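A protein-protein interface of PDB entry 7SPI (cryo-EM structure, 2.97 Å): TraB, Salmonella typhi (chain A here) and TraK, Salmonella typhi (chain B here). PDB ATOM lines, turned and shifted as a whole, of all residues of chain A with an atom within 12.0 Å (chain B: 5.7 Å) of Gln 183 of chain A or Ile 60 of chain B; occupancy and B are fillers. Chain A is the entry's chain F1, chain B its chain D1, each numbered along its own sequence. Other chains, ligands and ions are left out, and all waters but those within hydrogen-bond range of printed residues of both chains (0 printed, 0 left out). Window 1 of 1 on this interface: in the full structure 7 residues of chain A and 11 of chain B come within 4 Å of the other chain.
O of Thr 58 of chain B sits at hydrogen-bond distance from N of Phe 185 of chain A, at 2.7 Å. O of Ile 60 of chain B sits close to OG of Ser 182 of chain A (3.3 Å). O of Ile 60 of chain B lies within hydrogen-bond range of N of Gln 183 of chain A (3.1 Å). The side-chain hydroxyl (OG) of Ser 182 of chain A is in hydrogen-bond range of the side-chain hydroxyl (OG1) of Thr 61 of chain B, 2.9 Å away. N of Ala 62 of chain B lies within hydrogen-bond range of O of Asp 181 of chain A, at 3.2 Å. NZ of Lys 70 of chain B sits close to N of Gln 183 of chain A (3.2 Å).
The backbone carbonyl oxygen (O) of Glu 93 of chain B sits at hydrogen-bond distance from the backbone NH (N) of Thr 58 of chain B (2.8 Å). N of Glu 93 of chain B lies within hydrogen-bond range of O of Ala 59 of chain B (3.0 Å). The backbone NH (N) of Phe 91 of chain B sits at hydrogen-bond distance from the backbone carbonyl oxygen (O) of Thr 61 of chain B, at 2.9 Å.
Met 180 of chain A touches Ala 62 of chain B. O of Asp 181 of chain A touches CA of Thr 61 of chain B, 3.3 Å away. NZ of Lys 70 of chain B touches C of Ser 182 of chain A (3.8 Å). Gln 183 of chain A touches Thr 58 of chain B. Gln 183 of chain A touches Ala 59 of chain B (O to CA, 3.3 Å). Glu 184 of chain A touches Thr 58 of chain B (CA to O, 3.2 Å). Ala 59 of chain B touches Glu 184 of chain A. Phe 185 of chain A touches Val 57 of chain B (CD2 to O, 3.8 Å). Phe 185 of chain A touches Ile 60 of chain B (CE2 to CG2, 3.7 Å). Phe 185 of chain A touches Val 78 of chain B (CE2 to CG1, 3.4 Å).
Gln 183 of chain A touches just these residues of chain B: Thr 58 (3.9 Å), Ala 59 (3.3 Å), Ile 60 (3.1 Å) and Lys 70 (3.2 Å). Ile 60 of chain B touches just these residues of chain A: Ser 182, Gln 183 and Phe 185. Of chain A, only Gln 183 and Glu 184 come within 4 Å of Ala 59 of chain B. Ala 62 of chain B touches two residues of chain A. Val 78 of chain B touches just one residue of chain A: Phe 185 (3.4 Å). Val 92 of chain B touches none of the printed residues of chain A. Of the printed residues of chain A, Thr 58 of chain B touches Gln 183, Glu 184 and Phe 185. Of the printed residues of chain B, Asp 181 of chain A touches Thr 61 and Ala 62. Of the printed residues of chain B, Met 180 of chain A touches Ala 62. Printed residues of chain B within 4 Å of Glu 184 of chain A: Thr 58 (3.2 Å) and Ala 59 (3.8 Å). Printed residues of chain B within 4 Å of Ser 182 of chain A: Ile 60 (3.2 Å), Thr 61 (2.9 Å) and Lys 70 (3.8 Å). Phe 91 of chain B touches none of the printed residues of chain A. The nearest residue of chain B that does not touch Gln 183 of chain A is Thr 61 of chain B (5.3 Å).
Hydrophobic or aromatic side chains of chain A within 4 Å of the printed part of chain B: Met 180 and Phe 185. Of the 14 printed residues of chain B, 8 touch a printed residue of chain A. Hydrophobic or aromatic side chains of chain B within 4 Å of the printed part of chain A: Ala 59, Ile 60 and Val 78. Among the printed residues, 16 pairs touch across the chains.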
ATOM      1  N   MET A 179     -28.188   0.672   3.376  1.00  0.00           N
ATOM      2  CA  MET A 179     -26.869   0.152   2.943  1.00  0.00           C
ATOM      3  C   MET A 179     -27.055  -1.288   2.485  1.00  0.00           C
ATOM      4  O   MET A 179     -28.107  -1.879   2.793  1.00  0.00           O
ATOM      5  CB  MET A 179     -25.885   0.151   4.110  1.00  0.00           C
ATOM      6  CG  MET A 179     -24.597   0.888   3.826  1.00  0.00           C
ATOM      7  SD  MET A 179     -24.850   2.673   3.716  1.00  0.00           S
ATOM      8  CE  MET A 179     -25.638   2.996   5.292  1.00  0.00           C
ATOM      9  N   MET A 180     -26.066  -1.830   1.778  1.00  0.00           N
ATOM     10  CA  MET A 180     -26.232  -3.184   1.208  1.00  0.00           C
ATOM     11  C   MET A 180     -24.930  -3.958   1.372  1.00  0.00           C
ATOM     12  O   MET A 180     -23.858  -3.369   1.150  1.00  0.00           O
ATOM     13  CB  MET A 180     -26.595  -3.099  -0.274  1.00  0.00           C
ATOM     14  CG  MET A 180     -25.670  -2.202  -1.072  1.00  0.00           C
ATOM     15  SD  MET A 180     -26.379  -1.611  -2.626  1.00  0.00           S
ATOM     16  CE  MET A 180     -24.885  -1.112  -3.478  1.00  0.00           C
ATOM     17  N   ASP A 181     -25.038  -5.221   1.775  1.00  0.00           N
ATOM     18  CA  ASP A 181     -23.832  -6.072   1.889  1.00  0.00           C
ATOM     19  C   ASP A 181     -23.554  -6.708   0.534  1.00  0.00           C
ATOM     20  O   ASP A 181     -24.504  -7.140  -0.126  1.00  0.00           O
ATOM     21  CB  ASP A 181     -23.986  -7.131   2.976  1.00  0.00           C
ATOM     22  CG  ASP A 181     -25.239  -7.978   2.838  1.00  0.00           C
ATOM     23  OD1 ASP A 181     -26.336  -7.403   2.894  1.00  0.00           O
ATOM     24  OD2 ASP A 181     -25.104  -9.210   2.690  1.00  0.00           O
ATOM     25  N   SER A 182     -22.285  -6.768   0.159  1.00  0.00           N
ATOM     26  CA  SER A 182     -21.898  -7.367  -1.135  1.00  0.00           C
ATOM     27  C   SER A 182     -20.528  -8.015  -0.965  1.00  0.00           C
ATOM     28  O   SER A 182     -19.637  -7.340  -0.429  1.00  0.00           O
ATOM     29  CB  SER A 182     -21.858  -6.307  -2.189  1.00  0.00           C
ATOM     30  OG  SER A 182     -21.520  -6.856  -3.452  1.00  0.00           O
ATOM     31  N   GLN A 183     -20.359  -9.256  -1.417  1.00  0.00           N
ATOM     32  CA  GLN A 183     -19.020  -9.894  -1.338  1.00  0.00           C
ATOM     33  C   GLN A 183     -18.567 -10.301  -2.729  1.00  0.00           C
ATOM     34  O   GLN A 183     -19.394 -10.798  -3.492  1.00  0.00           O
ATOM     35  CB  GLN A 183     -19.031 -11.107  -0.413  1.00  0.00           C
ATOM     36  CG  GLN A 183     -17.657 -11.708  -0.175  1.00  0.00           C
ATOM     37  CD  GLN A 183     -17.723 -12.846   0.811  1.00  0.00           C
ATOM     38  OE1 GLN A 183     -18.714 -13.027   1.514  1.00  0.00           O
ATOM     39  NE2 GLN A 183     -16.656 -13.624   0.871  1.00  0.00           N
ATOM     40  N   GLU A 184     -17.294 -10.072  -3.023  1.00  0.00           N
ATOM     41  CA  GLU A 184     -16.730 -10.437  -4.338  1.00  0.00           C
ATOM     42  C   GLU A 184     -15.841 -11.653  -4.135  1.00  0.00           C
ATOM     43  O   GLU A 184     -14.941 -11.587  -3.286  1.00  0.00           O
ATOM     44  CB  GLU A 184     -15.907  -9.276  -4.880  1.00  0.00           C
ATOM     45  CG  GLU A 184     -15.989  -9.121  -6.383  1.00  0.00           C
ATOM     46  CD  GLU A 184     -17.012  -8.099  -6.842  1.00  0.00           C
ATOM     47  OE1 GLU A 184     -17.228  -7.990  -8.064  1.00  0.00           O
ATOM     48  OE2 GLU A 184     -17.590  -7.411  -5.975  1.00  0.00           O
ATOM     49  N   PHE A 185     -16.078 -12.713  -4.895  1.00  0.00           N
ATOM     50  CA  PHE A 185     -15.313 -13.961  -4.680  1.00  0.00           C
ATOM     51  C   PHE A 185     -14.036 -13.945  -5.532  1.00  0.00           C
ATOM     52  O   PHE A 185     -14.130 -13.640  -6.733  1.00  0.00           O
ATOM     53  CB  PHE A 185     -16.267 -15.131  -4.912  1.00  0.00           C
ATOM     54  CG  PHE A 185     -17.489 -15.117  -4.031  1.00  0.00           C
ATOM     55  CD1 PHE A 185     -17.369 -15.154  -2.654  1.00  0.00           C
ATOM     56  CD2 PHE A 185     -18.758 -15.078  -4.579  1.00  0.00           C
ATOM     57  CE1 PHE A 185     -18.491 -15.146  -1.844  1.00  0.00           C
ATOM     58  CE2 PHE A 185     -19.877 -15.069  -3.768  1.00  0.00           C
ATOM     59  CZ  PHE A 185     -19.744 -15.104  -2.403  1.00  0.00           C
ATOM     60  N   SER A 186     -12.878 -14.253  -4.935  1.00  0.00           N
ATOM     61  CA  SER A 186     -11.589 -14.259  -5.606  1.00  0.00           C
ATOM     62  C   SER A 186     -11.567 -15.286  -6.736  1.00  0.00           C
ATOM     63  O   SER A 186     -12.317 -16.268  -6.739  1.00  0.00           O
ATOM     64  CB  SER A 186     -10.466 -14.551  -4.611  1.00  0.00           C
ATOM     65  OG  SER A 186      -9.244 -14.806  -5.281  1.00  0.00           O
ATOM     66  N   VAL B  57     -20.002 -17.606 -10.041  1.00  0.00           N
ATOM     67  CA  VAL B  57     -20.529 -16.451  -9.360  1.00  0.00           C
ATOM     68  C   VAL B  57     -19.345 -15.664  -8.872  1.00  0.00           C
ATOM     69  O   VAL B  57     -18.472 -16.208  -8.218  1.00  0.00           O
ATOM     70  CB  VAL B  57     -21.389 -16.857  -8.169  1.00  0.00           C
ATOM     71  CG1 VAL B  57     -22.193 -15.668  -7.675  1.00  0.00           C
ATOM     72  CG2 VAL B  57     -22.325 -17.980  -8.564  1.00  0.00           C
ATOM     73  N   THR B  58     -19.300 -14.383  -9.203  1.00  0.00           N
ATOM     74  CA  THR B  58     -18.206 -13.546  -8.759  1.00  0.00           C
ATOM     75  C   THR B  58     -18.655 -12.602  -7.656  1.00  0.00           C
ATOM     76  O   THR B  58     -17.841 -12.143  -6.865  1.00  0.00           O
ATOM     77  CB  THR B  58     -17.627 -12.755  -9.940  1.00  0.00           C
ATOM     78  OG1 THR B  58     -17.556 -13.605 -11.086  1.00  0.00           O
ATOM     79  CG2 THR B  58     -16.234 -12.237  -9.623  1.00  0.00           C
ATOM     80  N   ALA B  59     -19.951 -12.332  -7.585  1.00  0.00           N
ATOM     81  CA  ALA B  59     -20.452 -11.416  -6.584  1.00  0.00           C
ATOM     82  C   ALA B  59     -21.884 -11.655  -6.187  1.00  0.00           C
ATOM     83  O   ALA B  59     -22.664 -12.158  -6.976  1.00  0.00           O
ATOM     84  CB  ALA B  59     -20.289 -10.001  -7.080  1.00  0.00           C
ATOM     85  N   ILE B  60     -22.241 -11.293  -4.962  1.00  0.00           N
ATOM     86  CA  ILE B  60     -23.626 -11.400  -4.518  1.00  0.00           C
ATOM     87  C   ILE B  60     -23.938 -10.188  -3.656  1.00  0.00           C
ATOM     88  O   ILE B  60     -23.089  -9.740  -2.897  1.00  0.00           O
ATOM     89  CB  ILE B  60     -23.879 -12.743  -3.804  1.00  0.00           C
ATOM     90  CG1 ILE B  60     -25.280 -12.815  -3.203  1.00  0.00           C
ATOM     91  CG2 ILE B  60     -22.796 -13.021  -2.774  1.00  0.00           C
ATOM     92  CD1 ILE B  60     -25.675 -14.214  -2.786  1.00  0.00           C
ATOM     93  N   THR B  61     -25.129  -9.623  -3.793  1.00  0.00           N
ATOM     94  CA  THR B  61     -25.528  -8.456  -3.019  1.00  0.00           C
ATOM     95  C   THR B  61     -26.935  -8.684  -2.528  1.00  0.00           C
ATOM     96  O   THR B  61     -27.767  -9.139  -3.285  1.00  0.00           O
ATOM     97  CB  THR B  61     -25.524  -7.197  -3.909  1.00  0.00           C
ATOM     98  OG1 THR B  61     -24.223  -7.018  -4.479  1.00  0.00           O
ATOM     99  CG2 THR B  61     -25.888  -5.956  -3.116  1.00  0.00           C
ATOM    100  N   ALA B  62     -27.231  -8.354  -1.284  1.00  0.00           N
ATOM    101  CA  ALA B  62     -28.599  -8.464  -0.796  1.00  0.00           C
ATOM    102  C   ALA B  62     -28.899  -7.306   0.136  1.00  0.00           C
ATOM    103  O   ALA B  62     -27.978  -6.669   0.622  1.00  0.00           O
ATOM    104  CB  ALA B  62     -28.791  -9.787  -0.091  1.00  0.00           C
ATOM    105  N   LEU B  67     -28.785 -11.712   4.465  1.00  0.00           N
ATOM    106  CA  LEU B  67     -28.054 -12.954   4.242  1.00  0.00           C
ATOM    107  C   LEU B  67     -26.978 -13.180   5.274  1.00  0.00           C
ATOM    108  O   LEU B  67     -25.994 -12.452   5.316  1.00  0.00           O
ATOM    109  CB  LEU B  67     -27.447 -12.995   2.840  1.00  0.00           C
ATOM    110  CG  LEU B  67     -28.402 -13.301   1.689  1.00  0.00           C
ATOM    111  CD1 LEU B  67     -27.614 -13.437   0.401  1.00  0.00           C
ATOM    112  CD2 LEU B  67     -29.171 -14.579   1.968  1.00  0.00           C
ATOM    113  N   LYS B  70     -22.248 -16.266   3.200  1.00  0.00           N
ATOM    114  CA  LYS B  70     -22.111 -16.536   1.773  1.00  0.00           C
ATOM    115  C   LYS B  70     -20.762 -17.150   1.432  1.00  0.00           C
ATOM    116  O   LYS B  70     -19.730 -16.548   1.696  1.00  0.00           O
ATOM    117  CB  LYS B  70     -22.292 -15.245   0.986  1.00  0.00           C
ATOM    118  CG  LYS B  70     -23.596 -14.516   1.271  1.00  0.00           C
ATOM    119  CD  LYS B  70     -23.557 -13.092   0.752  1.00  0.00           C
ATOM    120  CE  LYS B  70     -22.290 -12.383   1.200  1.00  0.00           C
ATOM    121  NZ  LYS B  70     -22.142 -11.057   0.542  1.00  0.00           N
ATOM    122  N   VAL B  78     -23.145 -20.494  -5.241  1.00  0.00           N
ATOM    123  CA  VAL B  78     -23.038 -19.804  -3.970  1.00  0.00           C
ATOM    124  C   VAL B  78     -23.859 -20.530  -2.948  1.00  0.00           C
ATOM    125  O   VAL B  78     -24.967 -20.964  -3.234  1.00  0.00           O
ATOM    126  CB  VAL B  78     -23.488 -18.331  -4.015  1.00  0.00           C
ATOM    127  CG1 VAL B  78     -22.291 -17.402  -4.084  1.00  0.00           C
ATOM    128  CG2 VAL B  78     -24.470 -18.080  -5.144  1.00  0.00           C
ATOM    129  N   PHE B  80     -25.700 -20.006   0.561  1.00  0.00           N
ATOM    130  CA  PHE B  80     -26.143 -18.887   1.380  1.00  0.00           C
ATOM    131  C   PHE B  80     -27.225 -19.241   2.388  1.00  0.00           C
ATOM    132  O   PHE B  80     -28.091 -20.063   2.118  1.00  0.00           O
ATOM    133  CB  PHE B  80     -26.576 -17.703   0.503  1.00  0.00           C
ATOM    134  CG  PHE B  80     -27.719 -17.997  -0.424  1.00  0.00           C
ATOM    135  CD1 PHE B  80     -27.486 -18.480  -1.693  1.00  0.00           C
ATOM    136  CD2 PHE B  80     -29.023 -17.749  -0.037  1.00  0.00           C
ATOM    137  CE1 PHE B  80     -28.531 -18.744  -2.546  1.00  0.00           C
ATOM    138  CE2 PHE B  80     -30.074 -18.007  -0.887  1.00  0.00           C
ATOM    139  CZ  PHE B  80     -29.828 -18.506  -2.146  1.00  0.00           C
ATOM    140  N   ILE B  90     -32.013 -10.324  -4.145  1.00  0.00           N
ATOM    141  CA  ILE B  90     -30.594 -10.645  -4.235  1.00  0.00           C
ATOM    142  C   ILE B  90     -30.103 -10.436  -5.659  1.00  0.00           C
ATOM    143  O   ILE B  90     -30.751 -10.884  -6.602  1.00  0.00           O
ATOM    144  CB  ILE B  90     -30.341 -12.123  -3.890  1.00  0.00           C
ATOM    145  CG1 ILE B  90     -31.337 -12.624  -2.847  1.00  0.00           C
ATOM    146  CG2 ILE B  90     -28.915 -12.330  -3.417  1.00  0.00           C
ATOM    147  CD1 ILE B  90     -31.107 -14.064  -2.444  1.00  0.00           C
ATOM    148  N   PHE B  91     -28.964  -9.769  -5.831  1.00  0.00           N
ATOM    149  CA  PHE B  91     -28.405  -9.599  -7.155  1.00  0.00           C
ATOM    150  C   PHE B  91     -27.150 -10.416  -7.289  1.00  0.00           C
ATOM    151  O   PHE B  91     -26.217 -10.229  -6.529  1.00  0.00           O
ATOM    152  CB  PHE B  91     -28.082  -8.134  -7.444  1.00  0.00           C
ATOM    153  CG  PHE B  91     -29.271  -7.319  -7.852  1.00  0.00           C
ATOM    154  CD1 PHE B  91     -30.076  -6.720  -6.903  1.00  0.00           C
ATOM    155  CD2 PHE B  91     -29.576  -7.148  -9.187  1.00  0.00           C
ATOM    156  CE1 PHE B  91     -31.169  -5.970  -7.279  1.00  0.00           C
ATOM    157  CE2 PHE B  91     -30.668  -6.398  -9.570  1.00  0.00           C
ATOM    158  CZ  PHE B  91     -31.468  -5.810  -8.613  1.00  0.00           C
ATOM    159  N   VAL B  92     -27.114 -11.307  -8.276  1.00  0.00           N
ATOM    160  CA  VAL B  92     -25.963 -12.167  -8.461  1.00  0.00           C
ATOM    161  C   VAL B  92     -25.240 -11.853  -9.750  1.00  0.00           C
ATOM    162  O   VAL B  92     -25.856 -11.701 -10.786  1.00  0.00           O
ATOM    163  CB  VAL B  92     -26.358 -13.651  -8.419  1.00  0.00           C
ATOM    164  CG1 VAL B  92     -26.338 -14.167  -6.991  1.00  0.00           C
ATOM    165  CG2 VAL B  92     -27.723 -13.866  -9.047  1.00  0.00           C
ATOM    166  N   GLU B  93     -23.927 -11.722  -9.682  1.00  0.00           N
ATOM    167  CA  GLU B  93     -23.147 -11.400 -10.855  1.00  0.00           C
ATOM    168  C   GLU B  93     -22.188 -12.492 -11.213  1.00  0.00           C
ATOM    169  O   GLU B  93     -21.357 -12.877 -10.407  1.00  0.00           O
ATOM    170  CB  GLU B  93     -22.344 -10.138 -10.598  1.00  0.00           C
ATOM    171  CG  GLU B  93     -21.577  -9.621 -11.799  1.00  0.00           C
ATOM    172  CD  GLU B  93     -20.696  -8.442 -11.444  1.00  0.00           C
ATOM    173  OE1 GLU B  93     -20.652  -8.075 -10.252  1.00  0.00           O
ATOM    174  OE2 GLU B  93     -20.048  -7.885 -12.356  1.00  0.00           O
